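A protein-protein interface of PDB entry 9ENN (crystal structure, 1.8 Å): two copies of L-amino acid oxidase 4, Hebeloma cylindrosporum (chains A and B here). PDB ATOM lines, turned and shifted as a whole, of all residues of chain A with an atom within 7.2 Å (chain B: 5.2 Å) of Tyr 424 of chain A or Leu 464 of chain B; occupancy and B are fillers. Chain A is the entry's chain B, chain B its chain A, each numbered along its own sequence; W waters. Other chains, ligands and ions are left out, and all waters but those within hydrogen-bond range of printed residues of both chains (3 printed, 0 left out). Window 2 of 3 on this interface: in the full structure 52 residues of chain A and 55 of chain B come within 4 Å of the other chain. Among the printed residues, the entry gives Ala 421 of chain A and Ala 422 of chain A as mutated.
The side-chain hydroxyl (OG) of Ser 415 of chain A is in hydrogen-bond range of the backbone NH (N) of Asn 462 of chain B.
OG1 of Thr 465 of chain B is in hydrogen-bond range of ND2 of Asn 462 of chain B (3.2 Å). The side-chain sulfur (SD) of Met 466 of chain B sits at hydrogen-bond distance from the backbone NH (N) of Val 318 of chain B (3.8 Å). The side-chain amide oxygen (OD1) of Asn 462 of chain B sits close to the backbone NH (N) of Leu 464 of chain B (3.4 Å).
Ser 415 of chain A touches Pro 463 of chain B (O to CG, 3.4 Å). OG of Ser 415 of chain A touches CA of Met 466 of chain B, at 3.5 Å. Leu 416 of chain A touches Pro 463 of chain B. Tyr 424 of chain A touches Pro 463 of chain B. Tyr 424 of chain A touches Leu 464 of chain B.
Of chain B, only Pro 463 and Leu 464 come within 4 Å of Tyr 424 of chain A. Of chain A, only Tyr 424 (3.98 Å) comes within 4 Å of Leu 464 of chain B. Printed residues of chain B within 4 Å of Ser 415 of chain A: Asn 462, Pro 463 and Met 466. Of the printed residues of chain A, Asn 462 of chain B touches Ser 415. Of the printed residues of chain A, Pro 463 of chain B touches Ser 415 (3.4 Å), Leu 416 (3.7 Å) and Tyr 424 (3.5 Å). The nearest printed residue of chain B that does not touch Ser 415 of chain A is Thr 465 of chain B (5.5 Å).
Of the 9 printed residues of chain B, 4 touch a printed residue of chain A. Among the printed residues, 6 pairs touch across the chains. Among the printed residues, no Asp or Glu carboxylate lies within 4 Å of a Lys or Arg side-chain nitrogen of the other chain.
No position is printed for both chains.
Water W2 bridges the side-chain hydroxyl (OG) of Ser 415 of chain A (2.6 Å) and the backbone carbonyl oxygen (O) of Met 466 of chain B (3.4 Å). Water W3 lies within hydrogen-bond range of O of Pro 463 of chain B (2.8 Å), NE2 of Gln 427 of chain A (3.0 Å) and SD of Met 466 of chain B (3.5 Å). Water W1 bridges OH of Tyr 424 of chain A (3.2 Å) and OD1 of Asn 462 of chain B (3.2 Å).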
ATOM      1  N   SER A 415       2.749 -14.436  31.476  1.00  0.00           N
ATOM      2  CA  SER A 415       3.756 -13.739  30.686  1.00  0.00           C
ATOM      3  C   SER A 415       3.150 -12.671  29.786  1.00  0.00           C
ATOM      4  O   SER A 415       3.860 -11.737  29.396  1.00  0.00           O
ATOM      5  CB  SER A 415       4.557 -14.724  29.833  1.00  0.00           C
ATOM      6  OG  SER A 415       5.688 -15.197  30.542  1.00  0.00           O
ATOM      7  N   LEU A 416       1.863 -12.775  29.454  1.00  0.00           N
ATOM      8  CA  LEU A 416       1.213 -11.801  28.590  1.00  0.00           C
ATOM      9  C   LEU A 416       0.527 -10.692  29.375  1.00  0.00           C
ATOM     10  O   LEU A 416      -0.021  -9.766  28.768  1.00  0.00           O
ATOM     11  CB  LEU A 416       0.180 -12.486  27.696  1.00  0.00           C
ATOM     12  CG  LEU A 416       0.755 -13.540  26.748  1.00  0.00           C
ATOM     13  CD1 LEU A 416      -0.342 -14.180  25.897  1.00  0.00           C
ATOM     14  CD2 LEU A 416       1.862 -12.965  25.888  1.00  0.00           C
ATOM     15  N   ILE A 417       0.560 -10.761  30.704  1.00  0.00           N
ATOM     16  CA  ILE A 417      -0.166  -9.848  31.576  1.00  0.00           C
ATOM     17  C   ILE A 417       0.824  -8.895  32.225  1.00  0.00           C
ATOM     18  O   ILE A 417       1.917  -9.301  32.634  1.00  0.00           O
ATOM     19  CB  ILE A 417      -0.977 -10.615  32.645  1.00  0.00           C
ATOM     20  CG1 ILE A 417      -2.095 -11.405  31.967  1.00  0.00           C
ATOM     21  CG2 ILE A 417      -1.459  -9.644  33.738  1.00  0.00           C
ATOM     22  CD1 ILE A 417      -2.779 -12.390  32.876  1.00  0.00           C
ATOM     23  N   THR A 419       2.663  -6.426  31.061  1.00  0.00           N
ATOM     24  CA  THR A 419       3.895  -6.069  30.377  1.00  0.00           C
ATOM     25  C   THR A 419       4.060  -4.562  30.240  1.00  0.00           C
ATOM     26  O   THR A 419       5.182  -4.090  30.026  1.00  0.00           O
ATOM     27  CB  THR A 419       3.964  -6.676  28.967  1.00  0.00           C
ATOM     28  OG1 THR A 419       2.989  -6.048  28.118  1.00  0.00           O
ATOM     29  CG2 THR A 419       3.743  -8.184  28.994  1.00  0.00           C
ATOM     30  N   GLY A 420       2.968  -3.804  30.299  1.00  0.00           N
ATOM     31  CA  GLY A 420       3.048  -2.386  30.046  1.00  0.00           C
ATOM     32  C   GLY A 420       3.199  -2.019  28.591  1.00  0.00           C
ATOM     33  O   GLY A 420       3.396  -0.836  28.285  1.00  0.00           O
ATOM     34  N   ALA A 421       3.159  -2.994  27.691  1.00  0.00           N
ATOM     35  CA  ALA A 421       3.440  -2.785  26.279  1.00  0.00           C
ATOM     36  C   ALA A 421       2.157  -2.984  25.486  1.00  0.00           C
ATOM     37  O   ALA A 421       1.526  -4.044  25.575  1.00  0.00           O
ATOM     38  CB  ALA A 421       4.527  -3.740  25.788  1.00  0.00           C
ATOM     39  N   ALA A 422       1.790  -1.969  24.700  1.00  0.00           N
ATOM     40  CA  ALA A 422       0.584  -2.045  23.883  1.00  0.00           C
ATOM     41  C   ALA A 422       0.561  -3.299  23.018  1.00  0.00           C
ATOM     42  O   ALA A 422      -0.492  -3.923  22.844  1.00  0.00           O
ATOM     43  CB  ALA A 422       0.477  -0.797  23.003  1.00  0.00           C
ATOM     44  N   THR A 423       1.710  -3.687  22.464  1.00  0.00           N
ATOM     45  CA  THR A 423       1.724  -4.801  21.523  1.00  0.00           C
ATOM     46  C   THR A 423       1.368  -6.119  22.209  1.00  0.00           C
ATOM     47  O   THR A 423       0.689  -6.968  21.617  1.00  0.00           O
ATOM     48  CB  THR A 423       3.088  -4.879  20.840  1.00  0.00           C
ATOM     49  OG1 THR A 423       3.127  -6.026  19.983  1.00  0.00           O
ATOM     50  CG2 THR A 423       4.215  -4.961  21.865  1.00  0.00           C
ATOM     51  N   TYR A 424       1.798  -6.312  23.455  1.00  0.00           N
ATOM     52  CA  TYR A 424       1.412  -7.525  24.166  1.00  0.00           C
ATOM     53  C   TYR A 424      -0.002  -7.419  24.723  1.00  0.00           C
ATOM     54  O   TYR A 424      -0.723  -8.423  24.753  1.00  0.00           O
ATOM     55  CB  TYR A 424       2.422  -7.813  25.275  1.00  0.00           C
ATOM     56  CG  TYR A 424       3.799  -8.134  24.725  1.00  0.00           C
ATOM     57  CD1 TYR A 424       3.956  -9.036  23.679  1.00  0.00           C
ATOM     58  CD2 TYR A 424       4.938  -7.518  25.230  1.00  0.00           C
ATOM     59  CE1 TYR A 424       5.212  -9.325  23.160  1.00  0.00           C
ATOM     60  CE2 TYR A 424       6.202  -7.804  24.717  1.00  0.00           C
ATOM     61  CZ  TYR A 424       6.331  -8.706  23.683  1.00  0.00           C
ATOM     62  OH  TYR A 424       7.582  -8.987  23.177  1.00  0.00           O
ATOM     63  N   GLU A 425      -0.436  -6.221  25.126  1.00  0.00           N
ATOM     64  CA  GLU A 425      -1.835  -6.047  25.502  1.00  0.00           C
ATOM     65  C   GLU A 425      -2.758  -6.413  24.348  1.00  0.00           C
ATOM     66  O   GLU A 425      -3.791  -7.064  24.550  1.00  0.00           O
ATOM     67  CB  GLU A 425      -2.089  -4.618  25.982  1.00  0.00           C
ATOM     68  CG  GLU A 425      -1.536  -4.346  27.377  1.00  0.00           C
ATOM     69  CD  GLU A 425      -2.260  -5.162  28.456  1.00  0.00           C
ATOM     70  OE1 GLU A 425      -3.507  -5.283  28.391  1.00  0.00           O
ATOM     71  OE2 GLU A 425      -1.582  -5.701  29.361  1.00  0.00           O
ATOM     72  N   GLU A 426      -2.390  -6.025  23.122  1.00  0.00           N
ATOM     73  CA  GLU A 426      -3.194  -6.380  21.958  1.00  0.00           C
ATOM     74  C   GLU A 426      -3.116  -7.875  21.662  1.00  0.00           C
ATOM     75  O   GLU A 426      -4.117  -8.488  21.273  1.00  0.00           O
ATOM     76  CB  GLU A 426      -2.739  -5.574  20.740  1.00  0.00           C
ATOM     77  CG  GLU A 426      -2.990  -4.081  20.854  1.00  0.00           C
ATOM     78  CD  GLU A 426      -2.283  -3.272  19.774  1.00  0.00           C
ATOM     79  OE1 GLU A 426      -1.891  -3.854  18.741  1.00  0.00           O
ATOM     80  OE2 GLU A 426      -2.116  -2.047  19.965  1.00  0.00           O
ATOM     81  N   GLN A 427      -1.930  -8.476  21.807  1.00  0.00           N
ATOM     82  CA  GLN A 427      -1.821  -9.920  21.635  1.00  0.00           C
ATOM     83  C   GLN A 427      -2.706 -10.648  22.634  1.00  0.00           C
ATOM     84  O   GLN A 427      -3.387 -11.623  22.291  1.00  0.00           O
ATOM     85  CB  GLN A 427      -0.365 -10.367  21.805  1.00  0.00           C
ATOM     86  CG  GLN A 427      -0.130 -11.859  21.573  1.00  0.00           C
ATOM     87  CD  GLN A 427       1.269 -12.328  21.982  1.00  0.00           C
ATOM     88  OE1 GLN A 427       2.135 -11.525  22.336  1.00  0.00           O
ATOM     89  NE2 GLN A 427       1.487 -13.636  21.935  1.00  0.00           N
ATOM     90  N   LEU A 428      -2.701 -10.190  23.884  1.00  0.00           N
ATOM     91  CA  LEU A 428      -3.489 -10.846  24.917  1.00  0.00           C
ATOM     92  C   LEU A 428      -4.974 -10.760  24.607  1.00  0.00           C
ATOM     93  O   LEU A 428      -5.701 -11.753  24.718  1.00  0.00           O
ATOM     94  CB  LEU A 428      -3.185 -10.220  26.272  1.00  0.00           C
ATOM     95  CG  LEU A 428      -4.034 -10.781  27.407  1.00  0.00           C
ATOM     96  CD1 LEU A 428      -3.756 -12.247  27.651  1.00  0.00           C
ATOM     97  CD2 LEU A 428      -3.778  -9.957  28.664  1.00  0.00           C
ATOM     98  N   GLU A 429      -5.445  -9.570  24.236  1.00  0.00           N
ATOM     99  CA  GLU A 429      -6.860  -9.406  23.939  1.00  0.00           C
ATOM    100  C   GLU A 429      -7.270 -10.294  22.777  1.00  0.00           C
ATOM    101  O   GLU A 429      -8.323 -10.940  22.818  1.00  0.00           O
ATOM    102  CB  GLU A 429      -7.161  -7.942  23.625  1.00  0.00           C
ATOM    103  CG  GLU A 429      -8.624  -7.645  23.379  1.00  0.00           C
ATOM    104  CD  GLU A 429      -8.830  -6.263  22.804  1.00  0.00           C
ATOM    105  OE1 GLU A 429      -8.504  -5.276  23.500  1.00  0.00           O
ATOM    106  OE2 GLU A 429      -9.313  -6.169  21.657  1.00  0.00           O
ATOM    107  N   HIS A 430      -6.436 -10.365  21.741  1.00  0.00           N
ATOM    108  CA  HIS A 430      -6.814 -11.146  20.575  1.00  0.00           C
ATOM    109  C   HIS A 430      -6.880 -12.629  20.913  1.00  0.00           C
ATOM    110  O   HIS A 430      -7.770 -13.343  20.435  1.00  0.00           O
ATOM    111  CB  HIS A 430      -5.832 -10.912  19.435  1.00  0.00           C
ATOM    112  CG  HIS A 430      -6.387 -11.283  18.100  1.00  0.00           C
ATOM    113  ND1 HIS A 430      -6.498 -12.589  17.676  1.00  0.00           N
ATOM    114  CD2 HIS A 430      -6.883 -10.519  17.100  1.00  0.00           C
ATOM    115  CE1 HIS A 430      -7.036 -12.613  16.470  1.00  0.00           C
ATOM    116  NE2 HIS A 430      -7.273 -11.370  16.094  1.00  0.00           N
ATOM    117  N   ALA B  42      10.161 -12.685  15.798  1.00  0.00           N
ATOM    118  CA  ALA B  42       9.207 -11.723  16.343  1.00  0.00           C
ATOM    119  C   ALA B  42       9.890 -10.429  16.768  1.00  0.00           C
ATOM    120  O   ALA B  42       9.322  -9.343  16.610  1.00  0.00           O
ATOM    121  CB  ALA B  42       8.466 -12.330  17.538  1.00  0.00           C
ATOM    122  N   SER B  43      11.104 -10.524  17.301  1.00  0.00           N
ATOM    123  CA  SER B  43      11.767  -9.398  17.931  1.00  0.00           C
ATOM    124  C   SER B  43      12.708  -8.705  16.944  1.00  0.00           C
ATOM    125  O   SER B  43      12.763  -9.038  15.756  1.00  0.00           O
ATOM    126  CB  SER B  43      12.535  -9.875  19.170  1.00  0.00           C
ATOM    127  OG  SER B  43      13.790 -10.439  18.805  1.00  0.00           O
ATOM    128  N   PRO B 315       8.783 -21.824  21.470  1.00  0.00           N
ATOM    129  CA  PRO B 315       8.447 -22.568  22.690  1.00  0.00           C
ATOM    130  C   PRO B 315       7.008 -23.063  22.642  1.00  0.00           C
ATOM    131  O   PRO B 315       6.132 -22.424  22.056  1.00  0.00           O
ATOM    132  CB  PRO B 315       8.652 -21.533  23.803  1.00  0.00           C
ATOM    133  CG  PRO B 315       9.684 -20.590  23.239  1.00  0.00           C
ATOM    134  CD  PRO B 315       9.368 -20.501  21.767  1.00  0.00           C
ATOM    135  N   VAL B 318       4.255 -20.736  23.538  1.00  0.00           N
ATOM    136  CA  VAL B 318       4.064 -19.765  22.466  1.00  0.00           C
ATOM    137  C   VAL B 318       3.190 -20.346  21.366  1.00  0.00           C
ATOM    138  O   VAL B 318       2.275 -19.682  20.869  1.00  0.00           O
ATOM    139  CB  VAL B 318       5.425 -19.305  21.915  1.00  0.00           C
ATOM    140  CG1 VAL B 318       5.244 -18.462  20.646  1.00  0.00           C
ATOM    141  CG2 VAL B 318       6.174 -18.510  22.969  1.00  0.00           C
ATOM    142  N   ASN B 462       7.881 -13.160  30.325  1.00  0.00           N
ATOM    143  CA  ASN B 462       8.486 -12.756  29.067  1.00  0.00           C
ATOM    144  C   ASN B 462       7.684 -13.373  27.932  1.00  0.00           C
ATOM    145  O   ASN B 462       7.705 -14.599  27.752  1.00  0.00           O
ATOM    146  CB  ASN B 462       9.936 -13.213  29.003  1.00  0.00           C
ATOM    147  CG  ASN B 462      10.604 -12.839  27.704  1.00  0.00           C
ATOM    148  OD1 ASN B 462      10.135 -11.962  26.974  1.00  0.00           O
ATOM    149  ND2 ASN B 462      11.663 -13.557  27.367  1.00  0.00           N
ATOM    150  N   PRO B 463       6.953 -12.566  27.160  1.00  0.00           N
ATOM    151  CA  PRO B 463       6.082 -13.138  26.122  1.00  0.00           C
ATOM    152  C   PRO B 463       6.812 -13.951  25.076  1.00  0.00           C
ATOM    153  O   PRO B 463       6.189 -14.815  24.444  1.00  0.00           O
ATOM    154  CB  PRO B 463       5.427 -11.899  25.486  1.00  0.00           C
ATOM    155  CG  PRO B 463       5.511 -10.847  26.538  1.00  0.00           C
ATOM    156  CD  PRO B 463       6.779 -11.109  27.295  1.00  0.00           C
ATOM    157  N   LEU B 464       8.103 -13.723  24.869  1.00  0.00           N
ATOM    158  CA  LEU B 464       8.820 -14.466  23.841  1.00  0.00           C
ATOM    159  C   LEU B 464       9.251 -15.858  24.286  1.00  0.00           C
ATOM    160  O   LEU B 464       9.664 -16.651  23.428  1.00  0.00           O
ATOM    161  CB  LEU B 464      10.039 -13.666  23.386  1.00  0.00           C
ATOM    162  CG  LEU B 464       9.693 -12.329  22.736  1.00  0.00           C
ATOM    163  CD1 LEU B 464      10.928 -11.505  22.501  1.00  0.00           C
ATOM    164  CD2 LEU B 464       8.977 -12.587  21.428  1.00  0.00           C
ATOM    165  N   THR B 465       9.170 -16.175  25.594  1.00  0.00           N
ATOM    166  CA  THR B 465       9.560 -17.493  26.091  1.00  0.00           C
ATOM    167  C   THR B 465       8.470 -18.173  26.909  1.00  0.00           C
ATOM    168  O   THR B 465       8.315 -19.399  26.818  1.00  0.00           O
ATOM    169  CB  THR B 465      10.849 -17.417  26.955  1.00  0.00           C
ATOM    170  OG1 THR B 465      10.693 -16.498  28.044  1.00  0.00           O
ATOM    171  CG2 THR B 465      12.033 -16.971  26.110  1.00  0.00           C
ATOM    172  N   MET B 466       7.725 -17.407  27.718  1.00  0.00           N
ATOM    173  CA  MET B 466       6.600 -17.911  28.512  1.00  0.00           C
ATOM    174  C   MET B 466       7.058 -19.051  29.418  1.00  0.00           C
ATOM    175  O   MET B 466       6.435 -20.113  29.499  1.00  0.00           O
ATOM    176  CB  MET B 466       5.444 -18.330  27.603  1.00  0.00           C
ATOM    177  CG  MET B 466       4.960 -17.214  26.684  1.00  0.00           C
ATOM    178  SD  MET B 466       3.542 -17.673  25.669  1.00  0.00           S
ATOM    179  CE  MET B 466       2.222 -17.517  26.871  1.00  0.00           C
HETATM  180  O   HOH W   1       9.744  -9.112  25.501  1.00  0.00           O
HETATM  181  O   HOH W   2       5.200 -17.587  31.417  1.00  0.00           O
HETATM  182  O   HOH W   3       3.693 -15.132  23.316  1.00  0.00           O
